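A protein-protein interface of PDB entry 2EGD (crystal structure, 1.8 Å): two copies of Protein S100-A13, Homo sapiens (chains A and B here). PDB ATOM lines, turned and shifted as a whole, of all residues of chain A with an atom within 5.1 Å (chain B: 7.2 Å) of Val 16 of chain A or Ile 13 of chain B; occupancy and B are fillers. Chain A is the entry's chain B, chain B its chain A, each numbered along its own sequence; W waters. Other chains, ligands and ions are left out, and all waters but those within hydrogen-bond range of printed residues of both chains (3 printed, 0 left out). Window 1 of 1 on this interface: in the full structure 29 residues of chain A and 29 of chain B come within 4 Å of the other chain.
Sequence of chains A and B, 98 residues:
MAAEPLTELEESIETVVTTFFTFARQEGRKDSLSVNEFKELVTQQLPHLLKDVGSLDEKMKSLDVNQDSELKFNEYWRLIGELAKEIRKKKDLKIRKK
The backbone NH (N) of Leu 49 of chain A is in hydrogen-bond range of the side-chain carboxylate (OE2) of Glu 10 of chain B.
OG1 of Thr 7 of chain B sits close to N of Leu 9 of chain B (3.5 Å).
O of Thr 15 of chain B sits at hydrogen-bond distance from OG1 of Thr 19 of chain B (2.8 Å).
The side-chain hydroxyl (OG) of Ser 12 of chain B lies within hydrogen-bond range of the backbone carbonyl oxygen (O) of Glu 8 of chain B, 3.0 Å away.
The backbone NH of Thr 7 of chain B sits at hydrogen-bond distance from the side-chain carboxylate of Glu 10 of chain B (3.0 Å).
The side-chain hydroxyl of Tyr 76 of chain A lies within hydrogen-bond range of the backbone carbonyl oxygen of Val 16 of chain A (2.6 Å).
OG1 of Thr 15 of chain B sits at hydrogen-bond distance from O of Glu 11 of chain B (3.1 Å).
Ser 12 of chain B touches Ser 12 of chain A.
CA of Val 16 of chain A touches CD1 of Leu 9 of chain B (3.8 Å).
Ala 84 of chain B touches Val 17 of chain A (O to CG2, 3.8 Å).
Glu 10 of chain B touches Leu 46 of chain A (OE2 to C, 3.2 Å).
Leu 9 of chain B touches Tyr 76 of chain A.
CZ2 of Trp 77 of chain B touches CZ2 of Trp 77 of chain A, at 3.5 Å.
CG2 of Ile 80 of chain B touches CH2 of Trp 77 of chain A, at 3.7 Å.
Trp 77 of chain A touches Ala 84 of chain B.
O of Ala 84 of chain A touches CG2 of Val 17 of chain B (3.7 Å).
Ala 84 of chain A touches Trp 77 of chain B.
Of the printed residues of chain B, Thr 19 of chain A touches Leu 9 (3.9 Å).
Of the printed residues of chain A, Glu 8 of chain B touches Thr 15 (3.9 Å).
Of the printed residues of chain A, Ile 13 of chain B touches Val 16, Ile 80, Ala 84 and Ile 87.
Of the printed residues of chain A, Thr 15 of chain B touches Ser 12.
The nearest printed residue of chain B that does not touch Thr 19 of chain A is Glu 8 of chain B (5.8 Å).
Of the 18 printed residues of chain A, 12 touch a printed residue of chain B.
Ser 12 of chain B touches its own counterpart, Ser 12 of chain A.
Trp 77 of chain A touches its own counterpart, Trp 77 of chain B.
Ile 80 of chain A touches Ile 13 of chain B, but with the chains exchanged Ile 13 of chain A does not touch Ile 80 of chain B (4.1 Å).
Ala 84 of chain A touches Ile 13 of chain B, but with the chains exchanged Ile 13 of chain A does not touch Ala 84 of chain B (4.3 Å).
Of the 24 pairs that touch across the chains among the printed residues, 10 have their exchanged pair printed and touching as well.
Water W3 lies within hydrogen-bond range of the side-chain hydroxyl of Thr 15 of chain B (2.6 Å), the side-chain hydroxyl of Ser 12 of chain A (3.1 Å) and the backbone carbonyl oxygen of Glu 11 of chain B (3.4 Å).
Water W1 lies within hydrogen-bond range of NE1 of Trp 77 of chain A (2.8 Å) and O of Trp 77 of chain B (2.9 Å).
Water W2 bridges the indole nitrogen (NE1) of Trp 77 of chain B and the backbone carbonyl oxygen (O) of Trp 77 of chain A.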
ATOM      1  N   SER A  12     -14.898  -5.455 -16.621  1.00  0.00           N
ATOM      2  CA  SER A  12     -15.856  -6.562 -16.769  1.00  0.00           C
ATOM      3  C   SER A  12     -17.007  -6.376 -15.801  1.00  0.00           C
ATOM      4  O   SER A  12     -18.157  -6.617 -16.172  1.00  0.00           O
ATOM      5  CB  SER A  12     -15.139  -7.884 -16.515  1.00  0.00           C
ATOM      6  OG  SER A  12     -14.374  -8.229 -17.675  1.00  0.00           O
ATOM      7  N   ILE A  13     -16.696  -5.973 -14.574  1.00  0.00           N
ATOM      8  CA  ILE A  13     -17.736  -5.770 -13.540  1.00  0.00           C
ATOM      9  C   ILE A  13     -18.595  -4.602 -14.033  1.00  0.00           C
ATOM     10  O   ILE A  13     -19.829  -4.690 -14.020  1.00  0.00           O
ATOM     11  CB  ILE A  13     -17.112  -5.413 -12.199  1.00  0.00           C
ATOM     12  CG1 ILE A  13     -16.313  -6.614 -11.676  1.00  0.00           C
ATOM     13  CG2 ILE A  13     -18.202  -5.065 -11.130  1.00  0.00           C
ATOM     14  CD1 ILE A  13     -15.443  -6.305 -10.496  1.00  0.00           C
ATOM     15  N   GLU A  14     -17.952  -3.553 -14.549  1.00  0.00           N
ATOM     16  CA  GLU A  14     -18.753  -2.440 -15.113  1.00  0.00           C
ATOM     17  C   GLU A  14     -19.670  -2.881 -16.252  1.00  0.00           C
ATOM     18  O   GLU A  14     -20.810  -2.420 -16.341  1.00  0.00           O
ATOM     19  CB  GLU A  14     -17.893  -1.218 -15.488  1.00  0.00           C
ATOM     20  CG  GLU A  14     -17.276  -0.475 -14.213  1.00  0.00           C
ATOM     21  CD  GLU A  14     -17.080   1.074 -14.385  1.00  0.00           C
ATOM     22  N   THR A  15     -19.198  -3.778 -17.127  1.00  0.00           N
ATOM     23  CA  THR A  15     -20.068  -4.286 -18.192  1.00  0.00           C
ATOM     24  C   THR A  15     -21.296  -5.034 -17.706  1.00  0.00           C
ATOM     25  O   THR A  15     -22.430  -4.863 -18.240  1.00  0.00           O
ATOM     26  CB  THR A  15     -19.280  -5.171 -19.184  1.00  0.00           C
ATOM     27  OG1 THR A  15     -18.365  -4.314 -19.902  1.00  0.00           O
ATOM     28  CG2 THR A  15     -20.243  -5.808 -20.236  1.00  0.00           C
ATOM     29  N   VAL A  16     -21.070  -5.877 -16.709  1.00  0.00           N
ATOM     30  CA  VAL A  16     -22.163  -6.630 -16.142  1.00  0.00           C
ATOM     31  C   VAL A  16     -23.217  -5.686 -15.592  1.00  0.00           C
ATOM     32  O   VAL A  16     -24.433  -5.901 -15.803  1.00  0.00           O
ATOM     33  CB  VAL A  16     -21.677  -7.658 -15.088  1.00  0.00           C
ATOM     34  CG1 VAL A  16     -22.877  -8.308 -14.372  1.00  0.00           C
ATOM     35  CG2 VAL A  16     -20.688  -8.732 -15.746  1.00  0.00           C
ATOM     36  N   VAL A  17     -22.785  -4.640 -14.899  1.00  0.00           N
ATOM     37  CA  VAL A  17     -23.765  -3.714 -14.330  1.00  0.00           C
ATOM     38  C   VAL A  17     -24.463  -2.887 -15.391  1.00  0.00           C
ATOM     39  O   VAL A  17     -25.687  -2.765 -15.394  1.00  0.00           O
ATOM     40  CB  VAL A  17     -23.128  -2.797 -13.266  1.00  0.00           C
ATOM     41  CG1 VAL A  17     -24.178  -1.818 -12.753  1.00  0.00           C
ATOM     42  CG2 VAL A  17     -22.636  -3.650 -12.108  1.00  0.00           C
ATOM     43  N   THR A  18     -23.676  -2.273 -16.263  1.00  0.00           N
ATOM     44  CA  THR A  18     -24.226  -1.469 -17.360  1.00  0.00           C
ATOM     45  C   THR A  18     -25.207  -2.203 -18.270  1.00  0.00           C
ATOM     46  O   THR A  18     -26.185  -1.591 -18.744  1.00  0.00           O
ATOM     47  CB  THR A  18     -23.110  -0.905 -18.235  1.00  0.00           C
ATOM     48  N   THR A  19     -24.938  -3.473 -18.576  1.00  0.00           N
ATOM     49  CA  THR A  19     -25.858  -4.228 -19.449  1.00  0.00           C
ATOM     50  C   THR A  19     -27.267  -4.245 -18.853  1.00  0.00           C
ATOM     51  O   THR A  19     -28.230  -4.039 -19.557  1.00  0.00           O
ATOM     52  CB  THR A  19     -25.361  -5.661 -19.707  1.00  0.00           C
ATOM     53  OG1 THR A  19     -24.024  -5.571 -20.247  1.00  0.00           O
ATOM     54  CG2 THR A  19     -26.261  -6.375 -20.742  1.00  0.00           C
ATOM     55  N   PHE A  20     -27.392  -4.464 -17.549  1.00  0.00           N
ATOM     56  CA  PHE A  20     -28.727  -4.366 -16.938  1.00  0.00           C
ATOM     57  C   PHE A  20     -29.490  -3.068 -17.282  1.00  0.00           C
ATOM     58  O   PHE A  20     -30.632  -3.092 -17.760  1.00  0.00           O
ATOM     59  CB  PHE A  20     -28.624  -4.482 -15.413  1.00  0.00           C
ATOM     60  CG  PHE A  20     -29.942  -4.291 -14.713  1.00  0.00           C
ATOM     61  CD1 PHE A  20     -30.818  -5.346 -14.580  1.00  0.00           C
ATOM     62  CD2 PHE A  20     -30.301  -3.060 -14.184  1.00  0.00           C
ATOM     63  CE1 PHE A  20     -32.012  -5.182 -13.898  1.00  0.00           C
ATOM     64  CE2 PHE A  20     -31.467  -2.891 -13.531  1.00  0.00           C
ATOM     65  CZ  PHE A  20     -32.341  -3.939 -13.373  1.00  0.00           C
ATOM     66  N   LEU A  46     -27.263 -13.054 -23.427  1.00  0.00           N
ATOM     67  CA  LEU A  46     -26.985 -14.359 -22.768  1.00  0.00           C
ATOM     68  C   LEU A  46     -27.393 -15.563 -23.600  1.00  0.00           C
ATOM     69  O   LEU A  46     -27.906 -16.554 -23.032  1.00  0.00           O
ATOM     70  CB  LEU A  46     -27.667 -14.412 -21.387  1.00  0.00           C
ATOM     71  CG  LEU A  46     -27.210 -13.335 -20.411  1.00  0.00           C
ATOM     72  CD1 LEU A  46     -28.087 -13.360 -19.161  1.00  0.00           C
ATOM     73  CD2 LEU A  46     -25.711 -13.533 -20.015  1.00  0.00           C
ATOM     74  N   LEU A  49     -24.924 -18.701 -22.599  1.00  0.00           N
ATOM     75  CA  LEU A  49     -24.969 -19.128 -21.217  1.00  0.00           C
ATOM     76  C   LEU A  49     -26.364 -19.576 -20.811  1.00  0.00           C
ATOM     77  O   LEU A  49     -26.472 -20.403 -19.923  1.00  0.00           O
ATOM     78  CB  LEU A  49     -24.450 -18.050 -20.288  1.00  0.00           C
ATOM     79  CG  LEU A  49     -22.970 -17.630 -20.453  1.00  0.00           C
ATOM     80  CD1 LEU A  49     -22.599 -16.631 -19.346  1.00  0.00           C
ATOM     81  CD2 LEU A  49     -21.981 -18.786 -20.452  1.00  0.00           C
ATOM     82  N   PHE A  73     -32.234  -4.702  -9.926  1.00  0.00           N
ATOM     83  CA  PHE A  73     -30.845  -5.140 -10.095  1.00  0.00           C
ATOM     84  C   PHE A  73     -30.464  -6.355  -9.245  1.00  0.00           C
ATOM     85  O   PHE A  73     -29.729  -7.246  -9.713  1.00  0.00           O
ATOM     86  CB  PHE A  73     -29.892  -3.973  -9.853  1.00  0.00           C
ATOM     87  CG  PHE A  73     -28.461  -4.340 -10.069  1.00  0.00           C
ATOM     88  CD1 PHE A  73     -27.869  -4.211 -11.321  1.00  0.00           C
ATOM     89  CD2 PHE A  73     -27.693  -4.867  -9.000  1.00  0.00           C
ATOM     90  CE1 PHE A  73     -26.559  -4.602 -11.538  1.00  0.00           C
ATOM     91  CE2 PHE A  73     -26.369  -5.280  -9.198  1.00  0.00           C
ATOM     92  CZ  PHE A  73     -25.786  -5.126 -10.474  1.00  0.00           C
ATOM     93  N   TYR A  76     -31.570  -9.443 -11.035  1.00  0.00           N
ATOM     94  CA  TYR A  76     -30.628  -9.711 -12.131  1.00  0.00           C
ATOM     95  C   TYR A  76     -29.292 -10.237 -11.625  1.00  0.00           C
ATOM     96  O   TYR A  76     -28.726 -11.167 -12.191  1.00  0.00           O
ATOM     97  CB  TYR A  76     -30.440  -8.436 -12.949  1.00  0.00           C
ATOM     98  CG  TYR A  76     -29.226  -8.327 -13.909  1.00  0.00           C
ATOM     99  CD1 TYR A  76     -29.269  -8.860 -15.191  1.00  0.00           C
ATOM    100  CD2 TYR A  76     -28.049  -7.641 -13.500  1.00  0.00           C
ATOM    101  CE1 TYR A  76     -28.168  -8.742 -16.061  1.00  0.00           C
ATOM    102  CE2 TYR A  76     -26.956  -7.488 -14.339  1.00  0.00           C
ATOM    103  CZ  TYR A  76     -27.018  -8.082 -15.626  1.00  0.00           C
ATOM    104  OH  TYR A  76     -25.978  -7.918 -16.503  1.00  0.00           O
ATOM    105  N   TRP A  77     -28.809  -9.686 -10.521  1.00  0.00           N
ATOM    106  CA  TRP A  77     -27.520 -10.109  -9.979  1.00  0.00           C
ATOM    107  C   TRP A  77     -27.556 -11.580  -9.544  1.00  0.00           C
ATOM    108  O   TRP A  77     -26.562 -12.293  -9.702  1.00  0.00           O
ATOM    109  CB  TRP A  77     -27.121  -9.213  -8.808  1.00  0.00           C
ATOM    110  CG  TRP A  77     -25.728  -9.538  -8.314  1.00  0.00           C
ATOM    111  CD1 TRP A  77     -25.382 -10.198  -7.161  1.00  0.00           C
ATOM    112  CD2 TRP A  77     -24.523  -9.309  -9.023  1.00  0.00           C
ATOM    113  NE1 TRP A  77     -24.013 -10.362  -7.098  1.00  0.00           N
ATOM    114  CE2 TRP A  77     -23.466  -9.843  -8.250  1.00  0.00           C
ATOM    115  CE3 TRP A  77     -24.230  -8.716 -10.268  1.00  0.00           C
ATOM    116  CZ2 TRP A  77     -22.123  -9.764  -8.658  1.00  0.00           C
ATOM    117  CZ3 TRP A  77     -22.920  -8.652 -10.678  1.00  0.00           C
ATOM    118  CH2 TRP A  77     -21.868  -9.163  -9.872  1.00  0.00           C
ATOM    119  N   ILE A  80     -26.892 -13.479 -12.613  1.00  0.00           N
ATOM    120  CA  ILE A  80     -25.478 -13.477 -12.951  1.00  0.00           C
ATOM    121  C   ILE A  80     -24.703 -14.439 -12.054  1.00  0.00           C
ATOM    122  O   ILE A  80     -23.800 -15.123 -12.539  1.00  0.00           O
ATOM    123  CB  ILE A  80     -24.866 -12.061 -12.895  1.00  0.00           C
ATOM    124  CG1 ILE A  80     -25.679 -11.099 -13.774  1.00  0.00           C
ATOM    125  CG2 ILE A  80     -23.372 -12.059 -13.195  1.00  0.00           C
ATOM    126  CD1 ILE A  80     -25.582 -11.359 -15.244  1.00  0.00           C
ATOM    127  N   LEU A  83     -25.120 -17.992 -13.278  1.00  0.00           N
ATOM    128  CA  LEU A  83     -24.317 -18.185 -14.481  1.00  0.00           C
ATOM    129  C   LEU A  83     -22.845 -18.288 -14.098  1.00  0.00           C
ATOM    130  O   LEU A  83     -22.121 -19.193 -14.579  1.00  0.00           O
ATOM    131  CB  LEU A  83     -24.540 -17.021 -15.438  1.00  0.00           C
ATOM    132  CG  LEU A  83     -25.984 -16.867 -15.939  1.00  0.00           C
ATOM    133  CD1 LEU A  83     -26.008 -15.732 -16.945  1.00  0.00           C
ATOM    134  CD2 LEU A  83     -26.464 -18.120 -16.592  1.00  0.00           C
ATOM    135  N   ALA A  84     -22.418 -17.417 -13.192  1.00  0.00           N
ATOM    136  CA  ALA A  84     -21.030 -17.494 -12.718  1.00  0.00           C
ATOM    137  C   ALA A  84     -20.696 -18.834 -12.084  1.00  0.00           C
ATOM    138  O   ALA A  84     -19.592 -19.346 -12.278  1.00  0.00           O
ATOM    139  CB  ALA A  84     -20.709 -16.342 -11.785  1.00  0.00           C
ATOM    140  N   ILE A  87     -19.932 -21.332 -14.752  1.00  0.00           N
ATOM    141  CA  ILE A  87     -18.597 -21.076 -15.272  1.00  0.00           C
ATOM    142  C   ILE A  87     -17.549 -21.549 -14.304  1.00  0.00           C
ATOM    143  O   ILE A  87     -16.550 -22.088 -14.734  1.00  0.00           O
ATOM    144  CB  ILE A  87     -18.351 -19.568 -15.654  1.00  0.00           C
ATOM    145  CG1 ILE A  87     -19.367 -19.138 -16.731  1.00  0.00           C
ATOM    146  CG2 ILE A  87     -16.890 -19.326 -16.086  1.00  0.00           C
ATOM    147  CD1 ILE A  87     -19.401 -17.653 -17.047  1.00  0.00           C
ATOM    148  N   LEU B   6     -18.339 -15.554 -27.263  1.00  0.00           N
ATOM    149  CA  LEU B   6     -19.244 -15.110 -26.194  1.00  0.00           C
ATOM    150  C   LEU B   6     -19.644 -13.675 -26.444  1.00  0.00           C
ATOM    151  O   LEU B   6     -18.901 -12.973 -27.111  1.00  0.00           O
ATOM    152  CB  LEU B   6     -18.553 -15.234 -24.838  1.00  0.00           C
ATOM    153  CG  LEU B   6     -18.367 -16.664 -24.292  1.00  0.00           C
ATOM    154  CD1 LEU B   6     -17.572 -16.630 -22.955  1.00  0.00           C
ATOM    155  CD2 LEU B   6     -19.682 -17.466 -24.131  1.00  0.00           C
ATOM    156  N   THR B   7     -20.810 -13.248 -25.933  1.00  0.00           N
ATOM    157  CA  THR B   7     -21.228 -11.848 -26.050  1.00  0.00           C
ATOM    158  C   THR B   7     -20.403 -10.995 -25.076  1.00  0.00           C
ATOM    159  O   THR B   7     -19.591 -11.530 -24.321  1.00  0.00           O
ATOM    160  CB  THR B   7     -22.688 -11.657 -25.703  1.00  0.00           C
ATOM    161  OG1 THR B   7     -22.868 -12.014 -24.323  1.00  0.00           O
ATOM    162  CG2 THR B   7     -23.604 -12.469 -26.637  1.00  0.00           C
ATOM    163  N   GLU B   8     -20.570  -9.672 -25.139  1.00  0.00           N
ATOM    164  CA  GLU B   8     -19.849  -8.775 -24.230  1.00  0.00           C
ATOM    165  C   GLU B   8     -20.206  -9.121 -22.801  1.00  0.00           C
ATOM    166  O   GLU B   8     -19.310  -9.179 -21.931  1.00  0.00           O
ATOM    167  CB  GLU B   8     -20.125  -7.293 -24.549  1.00  0.00           C
ATOM    168  N   LEU B   9     -21.490  -9.372 -22.540  1.00  0.00           N
ATOM    169  CA  LEU B   9     -21.896  -9.707 -21.152  1.00  0.00           C
ATOM    170  C   LEU B   9     -21.326 -11.066 -20.791  1.00  0.00           C
ATOM    171  O   LEU B   9     -20.763 -11.249 -19.718  1.00  0.00           O
ATOM    172  CB  LEU B   9     -23.411  -9.661 -20.997  1.00  0.00           C
ATOM    173  CG  LEU B   9     -23.985 -10.139 -19.676  1.00  0.00           C
ATOM    174  CD1 LEU B   9     -23.377  -9.285 -18.560  1.00  0.00           C
ATOM    175  CD2 LEU B   9     -25.555 -10.041 -19.705  1.00  0.00           C
ATOM    176  N   GLU B  10     -21.425 -12.036 -21.687  1.00  0.00           N
ATOM    177  CA  GLU B  10     -20.985 -13.375 -21.312  1.00  0.00           C
ATOM    178  C   GLU B  10     -19.470 -13.406 -21.038  1.00  0.00           C
ATOM    179  O   GLU B  10     -18.987 -14.065 -20.077  1.00  0.00           O
ATOM    180  CB  GLU B  10     -21.349 -14.393 -22.396  1.00  0.00           C
ATOM    181  CG  GLU B  10     -22.896 -14.646 -22.524  1.00  0.00           C
ATOM    182  CD  GLU B  10     -23.234 -15.449 -23.752  1.00  0.00           C
ATOM    183  OE1 GLU B  10     -22.494 -15.395 -24.767  1.00  0.00           O
ATOM    184  OE2 GLU B  10     -24.289 -16.151 -23.714  1.00  0.00           O
ATOM    185  N   GLU B  11     -18.718 -12.692 -21.874  1.00  0.00           N
ATOM    186  CA  GLU B  11     -17.267 -12.689 -21.749  1.00  0.00           C
ATOM    187  C   GLU B  11     -16.899 -11.978 -20.467  1.00  0.00           C
ATOM    188  O   GLU B  11     -15.937 -12.382 -19.776  1.00  0.00           O
ATOM    189  CB  GLU B  11     -16.624 -12.028 -22.965  1.00  0.00           C
ATOM    190  CG  GLU B  11     -15.152 -12.398 -23.166  1.00  0.00           C
ATOM    191  CD  GLU B  11     -14.608 -11.809 -24.434  1.00  0.00           C
ATOM    192  OE1 GLU B  11     -14.247 -12.589 -25.354  1.00  0.00           O
ATOM    193  OE2 GLU B  11     -14.565 -10.557 -24.528  1.00  0.00           O
ATOM    194  N   SER B  12     -17.667 -10.948 -20.099  1.00  0.00           N
ATOM    195  CA  SER B  12     -17.388 -10.238 -18.823  1.00  0.00           C
ATOM    196  C   SER B  12     -17.613 -11.107 -17.608  1.00  0.00           C
ATOM    197  O   SER B  12     -16.795 -11.078 -16.689  1.00  0.00           O
ATOM    198  CB  SER B  12     -18.200  -8.931 -18.679  1.00  0.00           C
ATOM    199  OG  SER B  12     -17.766  -7.990 -19.636  1.00  0.00           O
ATOM    200  N   ILE B  13     -18.681 -11.905 -17.608  1.00  0.00           N
ATOM    201  CA  ILE B  13     -18.913 -12.826 -16.483  1.00  0.00           C
ATOM    202  C   ILE B  13     -17.747 -13.829 -16.446  1.00  0.00           C
ATOM    203  O   ILE B  13     -17.160 -14.070 -15.354  1.00  0.00           O
ATOM    204  CB  ILE B  13     -20.247 -13.561 -16.547  1.00  0.00           C
ATOM    205  CG1 ILE B  13     -21.402 -12.533 -16.700  1.00  0.00           C
ATOM    206  CG2 ILE B  13     -20.399 -14.491 -15.279  1.00  0.00           C
ATOM    207  CD1 ILE B  13     -22.824 -13.144 -17.148  1.00  0.00           C
ATOM    208  N   GLU B  14     -17.350 -14.336 -17.617  1.00  0.00           N
ATOM    209  CA  GLU B  14     -16.274 -15.303 -17.654  1.00  0.00           C
ATOM    210  C   GLU B  14     -14.970 -14.705 -17.108  1.00  0.00           C
ATOM    211  O   GLU B  14     -14.222 -15.404 -16.398  1.00  0.00           O
ATOM    212  CB  GLU B  14     -16.032 -15.813 -19.076  1.00  0.00           C
ATOM    213  CG  GLU B  14     -14.901 -16.815 -19.200  1.00  0.00           C
ATOM    214  CD  GLU B  14     -14.606 -17.155 -20.661  1.00  0.00           C
ATOM    215  OE1 GLU B  14     -14.283 -16.210 -21.434  1.00  0.00           O
ATOM    216  OE2 GLU B  14     -14.720 -18.347 -21.033  1.00  0.00           O
ATOM    217  N   THR B  15     -14.672 -13.456 -17.471  1.00  0.00           N
ATOM    218  CA  THR B  15     -13.467 -12.751 -16.965  1.00  0.00           C
ATOM    219  C   THR B  15     -13.518 -12.641 -15.405  1.00  0.00           C
ATOM    220  O   THR B  15     -12.494 -12.856 -14.737  1.00  0.00           O
ATOM    221  CB  THR B  15     -13.310 -11.389 -17.641  1.00  0.00           C
ATOM    222  OG1 THR B  15     -13.059 -11.623 -19.044  1.00  0.00           O
ATOM    223  CG2 THR B  15     -12.107 -10.544 -17.029  1.00  0.00           C
ATOM    224  N   VAL B  16     -14.677 -12.296 -14.860  1.00  0.00           N
ATOM    225  CA  VAL B  16     -14.796 -12.182 -13.385  1.00  0.00           C
ATOM    226  C   VAL B  16     -14.418 -13.525 -12.749  1.00  0.00           C
ATOM    227  O   VAL B  16     -13.661 -13.583 -11.770  1.00  0.00           O
ATOM    228  CB  VAL B  16     -16.223 -11.725 -12.945  1.00  0.00           C
ATOM    229  CG1 VAL B  16     -16.424 -11.895 -11.428  1.00  0.00           C
ATOM    230  CG2 VAL B  16     -16.478 -10.271 -13.388  1.00  0.00           C
ATOM    231  N   VAL B  17     -14.934 -14.608 -13.326  1.00  0.00           N
ATOM    232  CA  VAL B  17     -14.659 -15.927 -12.752  1.00  0.00           C
ATOM    233  C   VAL B  17     -13.191 -16.309 -13.005  1.00  0.00           C
ATOM    234  O   VAL B  17     -12.507 -16.810 -12.103  1.00  0.00           O
ATOM    235  CB  VAL B  17     -15.598 -17.034 -13.303  1.00  0.00           C
ATOM    236  CG1 VAL B  17     -15.275 -18.358 -12.610  1.00  0.00           C
ATOM    237  CG2 VAL B  17     -17.073 -16.712 -12.984  1.00  0.00           C
ATOM    238  N   THR B  18     -12.699 -16.141 -14.238  1.00  0.00           N
ATOM    239  CA  THR B  18     -11.318 -16.482 -14.507  1.00  0.00           C
ATOM    240  C   THR B  18     -10.301 -15.762 -13.593  1.00  0.00           C
ATOM    241  O   THR B  18      -9.224 -16.301 -13.335  1.00  0.00           O
ATOM    242  CB  THR B  18     -10.976 -16.146 -15.990  1.00  0.00           C
ATOM    243  N   THR B  19     -10.593 -14.527 -13.192  1.00  0.00           N
ATOM    244  CA  THR B  19      -9.645 -13.729 -12.419  1.00  0.00           C
ATOM    245  C   THR B  19      -9.465 -14.393 -11.063  1.00  0.00           C
ATOM    246  O   THR B  19      -8.344 -14.461 -10.545  1.00  0.00           O
ATOM    247  CB  THR B  19     -10.127 -12.270 -12.291  1.00  0.00           C
ATOM    248  OG1 THR B  19     -10.154 -11.693 -13.627  1.00  0.00           O
ATOM    249  CG2 THR B  19      -9.150 -11.420 -11.394  1.00  0.00           C
ATOM    250  N   PHE B  73     -14.454 -19.478  -3.878  1.00  0.00           N
ATOM    251  CA  PHE B  73     -15.083 -18.672  -4.940  1.00  0.00           C
ATOM    252  C   PHE B  73     -16.351 -17.987  -4.398  1.00  0.00           C
ATOM    253  O   PHE B  73     -16.640 -16.828  -4.730  1.00  0.00           O
ATOM    254  CB  PHE B  73     -15.486 -19.550  -6.124  1.00  0.00           C
ATOM    255  CG  PHE B  73     -16.150 -18.775  -7.197  1.00  0.00           C
ATOM    256  CD1 PHE B  73     -15.395 -17.975  -8.049  1.00  0.00           C
ATOM    257  CD2 PHE B  73     -17.558 -18.767  -7.305  1.00  0.00           C
ATOM    258  CE1 PHE B  73     -16.027 -17.184  -9.034  1.00  0.00           C
ATOM    259  CE2 PHE B  73     -18.191 -17.994  -8.290  1.00  0.00           C
ATOM    260  CZ  PHE B  73     -17.429 -17.206  -9.152  1.00  0.00           C
ATOM    261  N   TRP B  77     -17.106 -14.087  -4.736  1.00  0.00           N
ATOM    262  CA  TRP B  77     -18.330 -13.650  -5.428  1.00  0.00           C
ATOM    263  C   TRP B  77     -19.110 -12.601  -4.597  1.00  0.00           C
ATOM    264  O   TRP B  77     -19.689 -11.647  -5.160  1.00  0.00           O
ATOM    265  CB  TRP B  77     -19.207 -14.855  -5.776  1.00  0.00           C
ATOM    266  CG  TRP B  77     -20.384 -14.383  -6.686  1.00  0.00           C
ATOM    267  CD1 TRP B  77     -21.722 -14.251  -6.344  1.00  0.00           C
ATOM    268  CD2 TRP B  77     -20.257 -13.922  -8.023  1.00  0.00           C
ATOM    269  NE1 TRP B  77     -22.416 -13.748  -7.422  1.00  0.00           N
ATOM    270  CE2 TRP B  77     -21.545 -13.546  -8.464  1.00  0.00           C
ATOM    271  CE3 TRP B  77     -19.170 -13.797  -8.906  1.00  0.00           C
ATOM    272  CZ2 TRP B  77     -21.789 -13.035  -9.732  1.00  0.00           C
ATOM    273  CZ3 TRP B  77     -19.424 -13.326 -10.226  1.00  0.00           C
ATOM    274  CH2 TRP B  77     -20.709 -12.943 -10.619  1.00  0.00           C
ATOM    275  N   ILE B  80     -17.492  -9.383  -5.249  1.00  0.00           N
ATOM    276  CA  ILE B  80     -17.889  -8.836  -6.565  1.00  0.00           C
ATOM    277  C   ILE B  80     -19.266  -8.177  -6.458  1.00  0.00           C
ATOM    278  O   ILE B  80     -19.521  -7.109  -7.034  1.00  0.00           O
ATOM    279  CB  ILE B  80     -17.856  -9.936  -7.688  1.00  0.00           C
ATOM    280  CG1 ILE B  80     -16.463 -10.586  -7.751  1.00  0.00           C
ATOM    281  CG2 ILE B  80     -18.210  -9.325  -9.067  1.00  0.00           C
ATOM    282  CD1 ILE B  80     -15.337  -9.540  -7.906  1.00  0.00           C
ATOM    283  N   ALA B  84     -20.294  -4.454  -7.429  1.00  0.00           N
ATOM    284  CA  ALA B  84     -21.412  -4.250  -8.381  1.00  0.00           C
ATOM    285  C   ALA B  84     -22.501  -3.331  -7.836  1.00  0.00           C
ATOM    286  O   ALA B  84     -23.002  -2.467  -8.548  1.00  0.00           O
ATOM    287  CB  ALA B  84     -22.031  -5.612  -8.892  1.00  0.00           C
HETATM  288  O   HOH W   1     -22.602 -11.405  -4.884  1.00  0.00           O
HETATM  289  O   HOH W   2     -25.279 -13.481  -7.322  1.00  0.00           O
HETATM  290  O   HOH W   3     -13.995  -9.644 -20.463  1.00  0.00           O
